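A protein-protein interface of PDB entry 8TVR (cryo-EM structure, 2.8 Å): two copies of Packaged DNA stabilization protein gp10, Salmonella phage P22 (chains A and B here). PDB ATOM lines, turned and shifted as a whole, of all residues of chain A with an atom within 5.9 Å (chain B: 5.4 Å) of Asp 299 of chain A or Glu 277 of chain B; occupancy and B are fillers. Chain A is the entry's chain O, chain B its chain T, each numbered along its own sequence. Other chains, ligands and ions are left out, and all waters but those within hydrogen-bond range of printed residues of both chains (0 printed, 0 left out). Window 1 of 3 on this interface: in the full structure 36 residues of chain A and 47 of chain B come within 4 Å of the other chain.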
ATOM      1  N   THR A  32       2.650 -14.721   5.811  1.00  0.00           N
ATOM      2  CA  THR A  32       3.817 -14.557   6.673  1.00  0.00           C
ATOM      3  C   THR A  32       5.069 -14.515   5.811  1.00  0.00           C
ATOM      4  O   THR A  32       5.459 -15.552   5.239  1.00  0.00           O
ATOM      5  CB  THR A  32       3.909 -15.696   7.687  1.00  0.00           C
ATOM      6  OG1 THR A  32       2.595 -16.025   8.157  1.00  0.00           O
ATOM      7  CG2 THR A  32       4.772 -15.285   8.866  1.00  0.00           C
ATOM      8  N   ARG A 297      -2.129  -8.314  17.517  1.00  0.00           N
ATOM      9  CA  ARG A 297      -0.673  -8.421  17.476  1.00  0.00           C
ATOM     10  C   ARG A 297      -0.283  -9.805  17.968  1.00  0.00           C
ATOM     11  O   ARG A 297      -0.529 -10.135  19.131  1.00  0.00           O
ATOM     12  CB  ARG A 297      -0.027  -7.333  18.330  1.00  0.00           C
ATOM     13  CG  ARG A 297       1.381  -6.965  17.917  1.00  0.00           C
ATOM     14  CD  ARG A 297       2.305  -6.882  19.121  1.00  0.00           C
ATOM     15  NE  ARG A 297       2.781  -8.196  19.537  1.00  0.00           N
ATOM     16  CZ  ARG A 297       3.720  -8.888  18.908  1.00  0.00           C
ATOM     17  NH1 ARG A 297       4.327  -8.415  17.832  1.00  0.00           N
ATOM     18  NH2 ARG A 297       4.060 -10.088  19.371  1.00  0.00           N
ATOM     19  N   PHE A 298       0.321 -10.607  17.092  1.00  0.00           N
ATOM     20  CA  PHE A 298       0.871 -11.889  17.523  1.00  0.00           C
ATOM     21  C   PHE A 298       1.810 -12.438  16.458  1.00  0.00           C
ATOM     22  O   PHE A 298       1.491 -12.408  15.268  1.00  0.00           O
ATOM     23  CB  PHE A 298      -0.231 -12.915  17.835  1.00  0.00           C
ATOM     24  CG  PHE A 298      -1.112 -13.255  16.663  1.00  0.00           C
ATOM     25  CD1 PHE A 298      -0.791 -14.300  15.812  1.00  0.00           C
ATOM     26  CD2 PHE A 298      -2.272 -12.539  16.424  1.00  0.00           C
ATOM     27  CE1 PHE A 298      -1.599 -14.611  14.740  1.00  0.00           C
ATOM     28  CE2 PHE A 298      -3.085 -12.851  15.357  1.00  0.00           C
ATOM     29  CZ  PHE A 298      -2.748 -13.887  14.513  1.00  0.00           C
ATOM     30  N   ASP A 299       2.958 -12.954  16.908  1.00  0.00           N
ATOM     31  CA  ASP A 299       3.952 -13.593  16.041  1.00  0.00           C
ATOM     32  C   ASP A 299       4.406 -12.652  14.928  1.00  0.00           C
ATOM     33  O   ASP A 299       4.417 -13.006  13.748  1.00  0.00           O
ATOM     34  CB  ASP A 299       3.415 -14.906  15.466  1.00  0.00           C
ATOM     35  CG  ASP A 299       2.916 -15.850  16.540  1.00  0.00           C
ATOM     36  OD1 ASP A 299       3.345 -15.708  17.704  1.00  0.00           O
ATOM     37  OD2 ASP A 299       2.093 -16.734  16.219  1.00  0.00           O
ATOM     38  N   SER A 300       4.771 -11.430  15.318  1.00  0.00           N
ATOM     39  CA  SER A 300       5.170 -10.350  14.418  1.00  0.00           C
ATOM     40  C   SER A 300       4.050  -9.925  13.477  1.00  0.00           C
ATOM     41  O   SER A 300       4.257  -9.049  12.630  1.00  0.00           O
ATOM     42  CB  SER A 300       6.422 -10.719  13.611  1.00  0.00           C
ATOM     43  OG  SER A 300       7.598 -10.543  14.383  1.00  0.00           O
ATOM     44  N   HIS A 301       2.869 -10.522  13.606  1.00  0.00           N
ATOM     45  CA  HIS A 301       1.699 -10.108  12.849  1.00  0.00           C
ATOM     46  C   HIS A 301       1.076  -8.887  13.511  1.00  0.00           C
ATOM     47  O   HIS A 301       0.758  -8.917  14.705  1.00  0.00           O
ATOM     48  CB  HIS A 301       0.677 -11.242  12.782  1.00  0.00           C
ATOM     49  CG  HIS A 301       0.903 -12.202  11.656  1.00  0.00           C
ATOM     50  ND1 HIS A 301       1.309 -11.800  10.403  1.00  0.00           N
ATOM     51  CD2 HIS A 301       0.769 -13.548  11.594  1.00  0.00           C
ATOM     52  CE1 HIS A 301       1.420 -12.855   9.618  1.00  0.00           C
ATOM     53  NE2 HIS A 301       1.098 -13.929  10.316  1.00  0.00           N
ATOM     54  N   PHE A 365      -4.390 -21.905  18.849  1.00  0.00           N
ATOM     55  CA  PHE A 365      -3.470 -21.811  17.721  1.00  0.00           C
ATOM     56  C   PHE A 365      -3.175 -23.135  17.027  1.00  0.00           C
ATOM     57  O   PHE A 365      -2.633 -23.119  15.917  1.00  0.00           O
ATOM     58  CB  PHE A 365      -2.142 -21.182  18.168  1.00  0.00           C
ATOM     59  CG  PHE A 365      -2.139 -19.683  18.126  1.00  0.00           C
ATOM     60  CD1 PHE A 365      -2.715 -18.947  19.148  1.00  0.00           C
ATOM     61  CD2 PHE A 365      -1.570 -19.008  17.061  1.00  0.00           C
ATOM     62  CE1 PHE A 365      -2.717 -17.569  19.109  1.00  0.00           C
ATOM     63  CE2 PHE A 365      -1.570 -17.629  17.019  1.00  0.00           C
ATOM     64  CZ  PHE A 365      -2.145 -16.909  18.044  1.00  0.00           C
ATOM     65  N   ASP B  20       3.623 -25.399  12.548  1.00  0.00           N
ATOM     66  CA  ASP B  20       4.051 -24.097  12.064  1.00  0.00           C
ATOM     67  C   ASP B  20       5.555 -24.093  11.813  1.00  0.00           C
ATOM     68  O   ASP B  20       6.297 -24.939  12.313  1.00  0.00           O
ATOM     69  CB  ASP B  20       3.679 -22.998  13.063  1.00  0.00           C
ATOM     70  CG  ASP B  20       3.737 -21.611  12.452  1.00  0.00           C
ATOM     71  OD1 ASP B  20       3.657 -21.501  11.211  1.00  0.00           O
ATOM     72  OD2 ASP B  20       3.862 -20.630  13.212  1.00  0.00           O
ATOM     73  N   ALA B 257       0.600  -8.874  22.389  1.00  0.00           N
ATOM     74  CA  ALA B 257       1.545  -9.951  22.644  1.00  0.00           C
ATOM     75  C   ALA B 257       2.948  -9.376  22.813  1.00  0.00           C
ATOM     76  O   ALA B 257       3.391  -8.575  21.978  1.00  0.00           O
ATOM     77  CB  ALA B 257       1.523 -10.969  21.507  1.00  0.00           C
ATOM     78  N   PRO B 258       3.668  -9.745  23.868  1.00  0.00           N
ATOM     79  CA  PRO B 258       4.967  -9.119  24.136  1.00  0.00           C
ATOM     80  C   PRO B 258       6.025  -9.502  23.113  1.00  0.00           C
ATOM     81  O   PRO B 258       5.961 -10.543  22.455  1.00  0.00           O
ATOM     82  CB  PRO B 258       5.334  -9.648  25.527  1.00  0.00           C
ATOM     83  CG  PRO B 258       4.040 -10.114  26.114  1.00  0.00           C
ATOM     84  CD  PRO B 258       3.253 -10.636  24.961  1.00  0.00           C
ATOM     85  N   SER B 259       7.014  -8.622  22.988  1.00  0.00           N
ATOM     86  CA  SER B 259       8.213  -8.877  22.201  1.00  0.00           C
ATOM     87  C   SER B 259       9.331  -7.997  22.753  1.00  0.00           C
ATOM     88  O   SER B 259       9.183  -7.365  23.801  1.00  0.00           O
ATOM     89  CB  SER B 259       7.950  -8.644  20.708  1.00  0.00           C
ATOM     90  OG  SER B 259       7.570  -7.307  20.453  1.00  0.00           O
ATOM     91  N   ALA B 272      12.898  -8.691  18.456  1.00  0.00           N
ATOM     92  CA  ALA B 272      12.620 -10.117  18.411  1.00  0.00           C
ATOM     93  C   ALA B 272      12.020 -10.518  17.068  1.00  0.00           C
ATOM     94  O   ALA B 272      11.398  -9.711  16.371  1.00  0.00           O
ATOM     95  CB  ALA B 272      11.672 -10.509  19.542  1.00  0.00           C
ATOM     96  N   THR B 273      12.216 -11.784  16.709  1.00  0.00           N
ATOM     97  CA  THR B 273      11.605 -12.364  15.526  1.00  0.00           C
ATOM     98  C   THR B 273      10.355 -13.142  15.929  1.00  0.00           C
ATOM     99  O   THR B 273       9.981 -13.196  17.101  1.00  0.00           O
ATOM    100  CB  THR B 273      12.601 -13.260  14.790  1.00  0.00           C
ATOM    101  OG1 THR B 273      12.930 -14.387  15.610  1.00  0.00           O
ATOM    102  CG2 THR B 273      13.869 -12.491  14.468  1.00  0.00           C
ATOM    103  N   ALA B 274       9.702 -13.765  14.945  1.00  0.00           N
ATOM    104  CA  ALA B 274       8.475 -14.507  15.226  1.00  0.00           C
ATOM    105  C   ALA B 274       8.725 -15.677  16.168  1.00  0.00           C
ATOM    106  O   ALA B 274       7.882 -15.975  17.022  1.00  0.00           O
ATOM    107  CB  ALA B 274       7.849 -14.997  13.921  1.00  0.00           C
ATOM    108  N   SER B 275       9.869 -16.350  16.033  1.00  0.00           N
ATOM    109  CA  SER B 275      10.191 -17.459  16.927  1.00  0.00           C
ATOM    110  C   SER B 275      10.425 -16.975  18.353  1.00  0.00           C
ATOM    111  O   SER B 275       9.984 -17.615  19.314  1.00  0.00           O
ATOM    112  CB  SER B 275      11.414 -18.209  16.404  1.00  0.00           C
ATOM    113  OG  SER B 275      11.289 -18.473  15.018  1.00  0.00           O
ATOM    114  N   ILE B 276      11.119 -15.847  18.511  1.00  0.00           N
ATOM    115  CA  ILE B 276      11.344 -15.297  19.843  1.00  0.00           C
ATOM    116  C   ILE B 276      10.027 -14.840  20.456  1.00  0.00           C
ATOM    117  O   ILE B 276       9.791 -15.008  21.659  1.00  0.00           O
ATOM    118  CB  ILE B 276      12.373 -14.154  19.782  1.00  0.00           C
ATOM    119  CG1 ILE B 276      13.657 -14.627  19.098  1.00  0.00           C
ATOM    120  CG2 ILE B 276      12.680 -13.637  21.176  1.00  0.00           C
ATOM    121  CD1 ILE B 276      14.428 -15.652  19.891  1.00  0.00           C
ATOM    122  N   GLU B 277       9.144 -14.265  19.638  1.00  0.00           N
ATOM    123  CA  GLU B 277       7.826 -13.876  20.124  1.00  0.00           C
ATOM    124  C   GLU B 277       7.017 -15.091  20.558  1.00  0.00           C
ATOM    125  O   GLU B 277       6.296 -15.036  21.557  1.00  0.00           O
ATOM    126  CB  GLU B 277       7.084 -13.084  19.051  1.00  0.00           C
ATOM    127  CG  GLU B 277       7.749 -11.770  18.700  1.00  0.00           C
ATOM    128  CD  GLU B 277       6.803 -10.802  18.030  1.00  0.00           C
ATOM    129  OE1 GLU B 277       5.601 -11.120  17.936  1.00  0.00           O
ATOM    130  OE2 GLU B 277       7.260  -9.721  17.603  1.00  0.00           O
ATOM    131  N   LYS B 278       7.121 -16.199  19.819  1.00  0.00           N
ATOM    132  CA  LYS B 278       6.443 -17.426  20.230  1.00  0.00           C
ATOM    133  C   LYS B 278       7.003 -17.957  21.545  1.00  0.00           C
ATOM    134  O   LYS B 278       6.244 -18.407  22.415  1.00  0.00           O
ATOM    135  CB  LYS B 278       6.561 -18.480  19.132  1.00  0.00           C
ATOM    136  CG  LYS B 278       5.559 -18.311  18.009  1.00  0.00           C
ATOM    137  CD  LYS B 278       6.043 -18.971  16.733  1.00  0.00           C
ATOM    138  CE  LYS B 278       5.289 -18.443  15.527  1.00  0.00           C
ATOM    139  NZ  LYS B 278       5.848 -18.963  14.253  1.00  0.00           N
ATOM    140  N   ILE B 279       8.327 -17.915  21.707  1.00  0.00           N
ATOM    141  CA  ILE B 279       8.940 -18.358  22.956  1.00  0.00           C
ATOM    142  C   ILE B 279       8.444 -17.510  24.120  1.00  0.00           C
ATOM    143  O   ILE B 279       8.107 -18.034  25.190  1.00  0.00           O
ATOM    144  CB  ILE B 279      10.477 -18.322  22.843  1.00  0.00           C
ATOM    145  CG1 ILE B 279      10.980 -19.500  22.010  1.00  0.00           C
ATOM    146  CG2 ILE B 279      11.121 -18.335  24.219  1.00  0.00           C
ATOM    147  CD1 ILE B 279      12.461 -19.443  21.710  1.00  0.00           C
ATOM    148  N   ILE B 280       8.386 -16.190  23.931  1.00  0.00           N
ATOM    149  CA  ILE B 280       7.871 -15.307  24.975  1.00  0.00           C
ATOM    150  C   ILE B 280       6.407 -15.619  25.266  1.00  0.00           C
ATOM    151  O   ILE B 280       5.987 -15.678  26.427  1.00  0.00           O
ATOM    152  CB  ILE B 280       8.065 -13.834  24.572  1.00  0.00           C
ATOM    153  CG1 ILE B 280       9.553 -13.496  24.472  1.00  0.00           C
ATOM    154  CG2 ILE B 280       7.376 -12.910  25.562  1.00  0.00           C
ATOM    155  CD1 ILE B 280       9.828 -12.151  23.841  1.00  0.00           C
ATOM    156  N   ARG B 281       5.611 -15.829  24.216  1.00  0.00           N
ATOM    157  CA  ARG B 281       4.194 -16.129  24.370  1.00  0.00           C
ATOM    158  C   ARG B 281       3.950 -17.457  25.069  1.00  0.00           C
ATOM    159  O   ARG B 281       2.865 -17.660  25.622  1.00  0.00           O
ATOM    160  CB  ARG B 281       3.517 -16.130  22.999  1.00  0.00           C
ATOM    161  CG  ARG B 281       2.017 -15.930  23.034  1.00  0.00           C
ATOM    162  CD  ARG B 281       1.505 -15.437  21.694  1.00  0.00           C
ATOM    163  NE  ARG B 281       2.019 -16.232  20.585  1.00  0.00           N
ATOM    164  CZ  ARG B 281       1.527 -17.406  20.212  1.00  0.00           C
ATOM    165  NH1 ARG B 281       0.510 -17.962  20.848  1.00  0.00           N
ATOM    166  NH2 ARG B 281       2.070 -18.036  19.174  1.00  0.00           N
ATOM    167  N   SER B 282       4.927 -18.366  25.054  1.00  0.00           N
ATOM    168  CA  SER B 282       4.780 -19.616  25.788  1.00  0.00           C
ATOM    169  C   SER B 282       4.761 -19.415  27.298  1.00  0.00           C
ATOM    170  O   SER B 282       4.406 -20.350  28.023  1.00  0.00           O
ATOM    171  CB  SER B 282       5.902 -20.585  25.411  1.00  0.00           C
ATOM    172  OG  SER B 282       7.172 -20.058  25.752  1.00  0.00           O
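The side-chain amino group of Lys 278 of chain B is in salt-bridge range of the side-chain carboxylate of Asp 20 of chain B, 2.8 Å away.
Printed residues of chain B within 4 Å of Asp 299 of chain A: Ala 274, Glu 277, Lys 278 and Arg 281. Printed residues of chain B within 4 Å of Ser 300 of chain A: Ala 274 (3.9 Å) and Glu 277 (2.8 Å). Of the printed residues of chain A, Ala 257 of chain B touches Arg 297. Ala 272 of chain B touches none of the printed residues of chain A. Thr 273 of chain B touches none of the printed residues of chain A. Of the printed residues of chain A, Glu 277 of chain B touches Arg 297, Asp 299 and Ser 300. Of the printed residues of chain A, Arg 281 of chain B touches Asp 299 and Phe 365. The nearest residue of chain A that does not touch Glu 277 of chain B is Phe 298 of chain A (4.3 Å).
The backbone carbonyl oxygen (O) of Ala 257 of chain B is in hydrogen-bond range of the guanidinium group (NE) of Arg 297 of chain A (2.5 Å). The guanidinium group (NH1) of Arg 297 of chain A is in salt-bridge range of the side-chain carboxylate (OE1) of Glu 277 of chain B (3.0 Å). The backbone NH (N) of Asp 299 of chain A lies within hydrogen-bond range of the side-chain carboxylate (OE1) of Glu 277 of chain B (3.4 Å). The side-chain carboxylate (OD1) of Asp 299 of chain A lies within salt-bridge range of the guanidinium group (NH2) of Arg 281 of chain B (3.0 Å). The backbone NH (N) of Ser 300 of chain A sits at hydrogen-bond distance from the side-chain carboxylate (OE1) of Glu 277 of chain B (2.8 Å).
NH2 of Arg 297 of chain A touches O of Pro 258 of chain B, 3.7 Å away. O of Asp 299 of chain A touches CB of Ala 274 of chain B, at 3.97 Å. Asp 299 of chain A touches Lys 278 of chain B (OD1 to CG, 3.4 Å). OG of Ser 300 of chain A touches N of Ala 274 of chain B, 3.9 Å away. Phe 365 of chain A touches Arg 281 of chain B (CE1 to NH1, 3.7 Å).
Of the 15 printed residues of chain B, 6 touch a printed residue of chain A. Hydrophobic or aromatic side chains of chain B that line the printed part of chain A: Ala 257 and Ala 274. Along chain B the printed residues that touch a printed residue of chain A span positions 257 to 281. Along chain A the printed residues that touch a printed residue of chain B span positions 297 to 365. Among the printed residues, 10 pairs touch across the chains. Among the printed residues, Asp or Glu carboxylates within 4 Å of a Lys or Arg side-chain nitrogen of the other chain: Arg 297 of chain A with Glu 277 of chain B (2.3 Å) and Asp 299 of chain A with Arg 281 of chain B (3.0 Å).
No position is printed for both chains.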
